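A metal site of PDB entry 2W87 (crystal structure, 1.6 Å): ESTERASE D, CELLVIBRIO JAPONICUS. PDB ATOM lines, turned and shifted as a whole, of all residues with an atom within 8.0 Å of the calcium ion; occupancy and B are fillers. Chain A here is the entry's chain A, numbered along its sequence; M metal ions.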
ATOM      1  N   LEU A   3     -25.035 -17.253 -11.040  1.00  0.00           N
ATOM      2  CA  LEU A   3     -23.652 -17.109 -11.470  1.00  0.00           C
ATOM      3  C   LEU A   3     -23.346 -18.164 -12.526  1.00  0.00           C
ATOM      4  O   LEU A   3     -23.303 -19.362 -12.239  1.00  0.00           O
ATOM      5  CB  LEU A   3     -22.681 -17.221 -10.295  1.00  0.00           C
ATOM      6  CG  LEU A   3     -21.189 -17.114 -10.614  1.00  0.00           C
ATOM      7  CD1 LEU A   3     -20.868 -15.817 -11.353  1.00  0.00           C
ATOM      8  CD2 LEU A   3     -20.348 -17.244  -9.335  1.00  0.00           C
ATOM      9  N   LEU A   4     -23.171 -17.700 -13.758  1.00  0.00           N
ATOM     10  CA  LEU A   4     -22.987 -18.592 -14.894  1.00  0.00           C
ATOM     11  C   LEU A   4     -21.519 -18.688 -15.256  1.00  0.00           C
ATOM     12  O   LEU A   4     -20.853 -17.688 -15.584  1.00  0.00           O
ATOM     13  CB  LEU A   4     -23.811 -18.121 -16.115  1.00  0.00           C
ATOM     14  CG  LEU A   4     -25.310 -17.956 -15.828  1.00  0.00           C
ATOM     15  CD1 LEU A   4     -25.988 -17.333 -17.024  1.00  0.00           C
ATOM     16  CD2 LEU A   4     -25.929 -19.317 -15.468  1.00  0.00           C
ATOM     17  N   GLN A   5     -21.037 -19.915 -15.160  1.00  0.00           N
ATOM     18  CA  GLN A   5     -19.678 -20.309 -15.512  1.00  0.00           C
ATOM     19  C   GLN A   5     -19.695 -21.163 -16.793  1.00  0.00           C
ATOM     20  O   GLN A   5     -20.655 -21.864 -17.061  1.00  0.00           O
ATOM     21  CB  GLN A   5     -19.043 -21.126 -14.394  1.00  0.00           C
ATOM     22  CG  GLN A   5     -18.914 -20.426 -13.052  1.00  0.00           C
ATOM     23  CD  GLN A   5     -17.790 -19.417 -12.995  1.00  0.00           C
ATOM     24  OE1 GLN A   5     -17.070 -19.235 -13.964  1.00  0.00           O
ATOM     25  NE2 GLN A   5     -17.607 -18.794 -11.827  1.00  0.00           N
ATOM     26  N   GLU A   6     -18.597 -21.111 -17.550  1.00  0.00           N
ATOM     27  CA  GLU A   6     -18.283 -22.128 -18.530  1.00  0.00           C
ATOM     28  C   GLU A   6     -18.516 -23.518 -17.963  1.00  0.00           C
ATOM     29  O   GLU A   6     -18.322 -23.748 -16.762  1.00  0.00           O
ATOM     30  CB  GLU A   6     -16.829 -21.988 -18.979  1.00  0.00           C
ATOM     31  CG  GLU A   6     -15.787 -22.240 -17.871  1.00  0.00           C
ATOM     32  CD  GLU A   6     -15.695 -21.125 -16.815  1.00  0.00           C
ATOM     33  OE1 GLU A   6     -16.009 -19.962 -17.158  1.00  0.00           O
ATOM     34  OE2 GLU A   6     -15.282 -21.392 -15.633  1.00  0.00           O
ATOM     35  N   ALA A   7     -18.950 -24.436 -18.830  1.00  0.00           N
ATOM     36  CA  ALA A   7     -19.066 -25.836 -18.477  1.00  0.00           C
ATOM     37  C   ALA A   7     -20.159 -26.075 -17.451  1.00  0.00           C
ATOM     38  O   ALA A   7     -20.113 -27.097 -16.742  1.00  0.00           O
ATOM     39  CB  ALA A   7     -17.766 -26.342 -17.942  1.00  0.00           C
ATOM     40  N   PHE A  11     -24.485 -21.752 -19.822  1.00  0.00           N
ATOM     41  CA  PHE A  11     -23.393 -21.337 -20.719  1.00  0.00           C
ATOM     42  C   PHE A  11     -23.635 -22.039 -22.049  1.00  0.00           C
ATOM     43  O   PHE A  11     -23.730 -23.270 -22.088  1.00  0.00           O
ATOM     44  CB  PHE A  11     -22.026 -21.699 -20.167  1.00  0.00           C
ATOM     45  CG  PHE A  11     -20.879 -21.132 -20.993  1.00  0.00           C
ATOM     46  CD1 PHE A  11     -20.349 -19.890 -20.684  1.00  0.00           C
ATOM     47  CD2 PHE A  11     -20.376 -21.812 -22.058  1.00  0.00           C
ATOM     48  CE1 PHE A  11     -19.294 -19.358 -21.394  1.00  0.00           C
ATOM     49  CE2 PHE A  11     -19.327 -21.264 -22.823  1.00  0.00           C
ATOM     50  CZ  PHE A  11     -18.804 -20.028 -22.485  1.00  0.00           C
ATOM     51  N   ILE A  18     -12.510 -22.395 -24.315  1.00  0.00           N
ATOM     52  CA  ILE A  18     -12.494 -22.257 -22.876  1.00  0.00           C
ATOM     53  C   ILE A  18     -11.088 -22.579 -22.372  1.00  0.00           C
ATOM     54  O   ILE A  18     -10.579 -23.669 -22.589  1.00  0.00           O
ATOM     55  CB  ILE A  18     -13.522 -23.162 -22.181  1.00  0.00           C
ATOM     56  CG1 ILE A  18     -14.901 -22.835 -22.701  1.00  0.00           C
ATOM     57  CG2 ILE A  18     -13.473 -22.958 -20.656  1.00  0.00           C
ATOM     58  CD1 ILE A  18     -15.369 -21.466 -22.288  1.00  0.00           C
ATOM     59  N   ASP A  19     -10.468 -21.609 -21.705  1.00  0.00           N
ATOM     60  CA  ASP A  19      -9.074 -21.688 -21.326  1.00  0.00           C
ATOM     61  C   ASP A  19      -8.939 -21.531 -19.819  1.00  0.00           C
ATOM     62  O   ASP A  19      -9.884 -21.124 -19.113  1.00  0.00           O
ATOM     63  CB  ASP A  19      -8.258 -20.574 -21.995  1.00  0.00           C
ATOM     64  CG  ASP A  19      -8.160 -20.705 -23.483  1.00  0.00           C
ATOM     65  OD1 ASP A  19      -8.716 -21.656 -24.073  1.00  0.00           O
ATOM     66  OD2 ASP A  19      -7.478 -19.836 -24.067  1.00  0.00           O
ATOM     67  N   GLY A  24      -6.643 -16.551 -11.781  1.00  0.00           N
ATOM     68  CA  GLY A  24      -7.550 -15.562 -11.185  1.00  0.00           C
ATOM     69  C   GLY A  24      -9.011 -15.717 -11.569  1.00  0.00           C
ATOM     70  O   GLY A  24      -9.847 -15.002 -11.051  1.00  0.00           O
ATOM     71  N   PHE A  25      -9.296 -16.653 -12.481  1.00  0.00           N
ATOM     72  CA  PHE A  25     -10.662 -16.951 -12.911  1.00  0.00           C
ATOM     73  C   PHE A  25     -11.351 -17.754 -11.804  1.00  0.00           C
ATOM     74  O   PHE A  25     -10.701 -18.183 -10.839  1.00  0.00           O
ATOM     75  CB  PHE A  25     -10.670 -17.776 -14.186  1.00  0.00           C
ATOM     76  CG  PHE A  25      -9.883 -19.059 -14.080  1.00  0.00           C
ATOM     77  CD1 PHE A  25     -10.451 -20.184 -13.530  1.00  0.00           C
ATOM     78  CD2 PHE A  25      -8.577 -19.107 -14.507  1.00  0.00           C
ATOM     79  CE1 PHE A  25      -9.724 -21.353 -13.387  1.00  0.00           C
ATOM     80  CE2 PHE A  25      -7.857 -20.256 -14.383  1.00  0.00           C
ATOM     81  CZ  PHE A  25      -8.463 -21.395 -13.832  1.00  0.00           C
ATOM     82  N   THR A  26     -12.652 -17.963 -11.968  1.00  0.00           N
ATOM     83  CA  THR A  26     -13.457 -18.759 -11.071  1.00  0.00           C
ATOM     84  C   THR A  26     -14.103 -19.866 -11.922  1.00  0.00           C
ATOM     85  O   THR A  26     -14.086 -19.783 -13.136  1.00  0.00           O
ATOM     86  CB  THR A  26     -14.492 -17.907 -10.324  1.00  0.00           C
ATOM     87  OG1 THR A  26     -15.321 -17.190 -11.237  1.00  0.00           O
ATOM     88  CG2 THR A  26     -13.793 -16.893  -9.411  1.00  0.00           C
ATOM     89  N   GLY A  27     -14.626 -20.920 -11.306  1.00  0.00           N
ATOM     90  CA  GLY A  27     -15.045 -22.066 -12.087  1.00  0.00           C
ATOM     91  C   GLY A  27     -13.868 -22.785 -12.711  1.00  0.00           C
ATOM     92  O   GLY A  27     -12.769 -22.720 -12.184  1.00  0.00           O
ATOM     93  N   SER A  28     -14.082 -23.489 -13.823  1.00  0.00           N
ATOM     94  CA  SER A  28     -13.028 -24.269 -14.430  1.00  0.00           C
ATOM     95  C   SER A  28     -12.181 -23.470 -15.435  1.00  0.00           C
ATOM     96  O   SER A  28     -11.186 -23.989 -15.982  1.00  0.00           O
ATOM     97  CB  SER A  28     -13.603 -25.510 -15.100  1.00  0.00           C
ATOM     98  OG  SER A  28     -14.606 -25.166 -16.044  1.00  0.00           O
ATOM     99  N   GLY A  29     -12.528 -22.208 -15.675  1.00  0.00           N
ATOM    100  CA  GLY A  29     -11.742 -21.402 -16.607  1.00  0.00           C
ATOM    101  C   GLY A  29     -12.408 -20.088 -17.012  1.00  0.00           C
ATOM    102  O   GLY A  29     -13.103 -19.457 -16.217  1.00  0.00           O
ATOM    103  N   PHE A  30     -12.175 -19.706 -18.257  1.00  0.00           N
ATOM    104  CA  PHE A  30     -12.728 -18.476 -18.815  1.00  0.00           C
ATOM    105  C   PHE A  30     -12.898 -18.657 -20.312  1.00  0.00           C
ATOM    106  O   PHE A  30     -12.255 -19.504 -20.920  1.00  0.00           O
ATOM    107  CB  PHE A  30     -11.808 -17.297 -18.513  1.00  0.00           C
ATOM    108  CG  PHE A  30     -10.367 -17.513 -18.893  1.00  0.00           C
ATOM    109  CD1 PHE A  30      -9.927 -17.260 -20.183  1.00  0.00           C
ATOM    110  CD2 PHE A  30      -9.438 -17.939 -17.962  1.00  0.00           C
ATOM    111  CE1 PHE A  30      -8.614 -17.443 -20.531  1.00  0.00           C
ATOM    112  CE2 PHE A  30      -8.117 -18.112 -18.302  1.00  0.00           C
ATOM    113  CZ  PHE A  30      -7.696 -17.865 -19.581  1.00  0.00           C
ATOM    114  N   ALA A  31     -13.826 -17.898 -20.880  1.00  0.00           N
ATOM    115  CA  ALA A  31     -14.067 -17.960 -22.321  1.00  0.00           C
ATOM    116  C   ALA A  31     -13.071 -17.009 -23.008  1.00  0.00           C
ATOM    117  O   ALA A  31     -12.998 -15.816 -22.684  1.00  0.00           O
ATOM    118  CB  ALA A  31     -15.507 -17.563 -22.639  1.00  0.00           C
ATOM    119  N   ARG A  58     -17.426 -10.549 -15.435  1.00  0.00           N
ATOM    120  CA  ARG A  58     -16.071 -10.535 -14.902  1.00  0.00           C
ATOM    121  C   ARG A  58     -15.101 -10.897 -16.024  1.00  0.00           C
ATOM    122  O   ARG A  58     -15.301 -11.887 -16.742  1.00  0.00           O
ATOM    123  CB  ARG A  58     -15.938 -11.513 -13.741  1.00  0.00           C
ATOM    124  CG  ARG A  58     -14.642 -11.352 -12.971  1.00  0.00           C
ATOM    125  CD  ARG A  58     -14.704 -12.057 -11.643  1.00  0.00           C
ATOM    126  NE  ARG A  58     -13.523 -11.792 -10.826  1.00  0.00           N
ATOM    127  CZ  ARG A  58     -12.457 -12.584 -10.756  1.00  0.00           C
ATOM    128  NH1 ARG A  58     -12.411 -13.712 -11.450  1.00  0.00           N
ATOM    129  NH2 ARG A  58     -11.437 -12.238  -9.992  1.00  0.00           N
ATOM    130  N   TRP A  94      -8.413  -9.310 -13.137  1.00  0.00           N
ATOM    131  CA  TRP A  94      -9.810  -9.400 -13.479  1.00  0.00           C
ATOM    132  C   TRP A  94     -10.557  -8.234 -12.902  1.00  0.00           C
ATOM    133  O   TRP A  94     -10.295  -7.800 -11.771  1.00  0.00           O
ATOM    134  CB  TRP A  94     -10.388 -10.709 -12.956  1.00  0.00           C
ATOM    135  CG  TRP A  94      -9.652 -11.897 -13.467  1.00  0.00           C
ATOM    136  CD1 TRP A  94      -8.507 -12.433 -12.977  1.00  0.00           C
ATOM    137  CD2 TRP A  94      -9.989 -12.678 -14.632  1.00  0.00           C
ATOM    138  NE1 TRP A  94      -8.114 -13.501 -13.734  1.00  0.00           N
ATOM    139  CE2 TRP A  94      -8.997 -13.673 -14.762  1.00  0.00           C
ATOM    140  CE3 TRP A  94     -11.027 -12.632 -15.563  1.00  0.00           C
ATOM    141  CZ2 TRP A  94      -9.012 -14.614 -15.796  1.00  0.00           C
ATOM    142  CZ3 TRP A  94     -11.051 -13.593 -16.604  1.00  0.00           C
ATOM    143  CH2 TRP A  94     -10.041 -14.556 -16.698  1.00  0.00           C
ATOM    144  N   ILE A 123     -13.412 -13.771 -20.693  1.00  0.00           N
ATOM    145  CA  ILE A 123     -14.629 -13.615 -19.875  1.00  0.00           C
ATOM    146  C   ILE A 123     -14.728 -14.735 -18.862  1.00  0.00           C
ATOM    147  O   ILE A 123     -14.880 -15.897 -19.209  1.00  0.00           O
ATOM    148  CB  ILE A 123     -15.916 -13.615 -20.745  1.00  0.00           C
ATOM    149  CG1 ILE A 123     -15.805 -12.581 -21.882  1.00  0.00           C
ATOM    150  CG2 ILE A 123     -17.167 -13.498 -19.870  1.00  0.00           C
ATOM    151  CD1 ILE A 123     -15.655 -11.144 -21.443  1.00  0.00           C
ATOM    152  N   ASP A 124     -14.672 -14.376 -17.591  1.00  0.00           N
ATOM    153  CA  ASP A 124     -14.681 -15.393 -16.530  1.00  0.00           C
ATOM    154  C   ASP A 124     -16.062 -15.917 -16.230  1.00  0.00           C
ATOM    155  O   ASP A 124     -16.247 -17.133 -16.071  1.00  0.00           O
ATOM    156  CB  ASP A 124     -14.102 -14.801 -15.256  1.00  0.00           C
ATOM    157  CG  ASP A 124     -14.083 -15.773 -14.107  1.00  0.00           C
ATOM    158  OD1 ASP A 124     -13.941 -16.989 -14.329  1.00  0.00           O
ATOM    159  OD2 ASP A 124     -14.161 -15.314 -12.953  1.00  0.00           O
ATOM    160  N   SER A 125     -17.001 -15.004 -16.120  1.00  0.00           N
ATOM    161  CA  SER A 125     -18.344 -15.337 -15.692  1.00  0.00           C
ATOM    162  C   SER A 125     -19.345 -14.233 -15.982  1.00  0.00           C
ATOM    163  O   SER A 125     -18.974 -13.067 -16.150  1.00  0.00           O
ATOM    164  CB  SER A 125     -18.324 -15.582 -14.206  1.00  0.00           C
ATOM    165  OG  SER A 125     -17.934 -14.417 -13.478  1.00  0.00           O
ATOM    166  N   LEU A 126     -20.628 -14.614 -15.921  1.00  0.00           N
ATOM    167  CA  LEU A 126     -21.729 -13.683 -15.982  1.00  0.00           C
ATOM    168  C   LEU A 126     -22.582 -13.915 -14.728  1.00  0.00           C
ATOM    169  O   LEU A 126     -22.997 -15.034 -14.473  1.00  0.00           O
ATOM    170  CB  LEU A 126     -22.596 -13.921 -17.230  1.00  0.00           C
ATOM    171  CG  LEU A 126     -23.868 -13.069 -17.325  1.00  0.00           C
ATOM    172  CD1 LEU A 126     -23.510 -11.601 -17.546  1.00  0.00           C
ATOM    173  CD2 LEU A 126     -24.817 -13.590 -18.392  1.00  0.00           C
HETATM  174 CA    CA M   1     -15.129 -18.945 -15.072  1.00  0.00          CA
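The side-chain carboxylate (OE2) of Glu 6 sits close to the backbone NH (N) of Ser 28, 3.0 Å away.
OD2 of Asp 124 is in salt-bridge range of NH1 of Arg 58 (2.8 Å).
Within 4 Å of the calcium ion: Gln 5, Glu 6, Thr 26, Gly 29 and Asp 124.
The calcium ion is bound by the side-chain amide oxygen (OE1) of Gln 5 (2.3 Å), the backbone carbonyl oxygen (O) of Asp 124 (2.4 Å), the backbone carbonyl oxygen (O) of Thr 26 (2.4 Å), the backbone carbonyl oxygen (O) of Gly 29 (2.4 Å), the side-chain carboxylate (OD1) of Asp 124 (2.4 Å), the side-chain carboxylate (OE1) of Glu 6 (2.5 Å) and the side-chain carboxylate (OE2) of Glu 6 (2.5 Å).
The calcium ion has seven donor atoms within binding distance.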
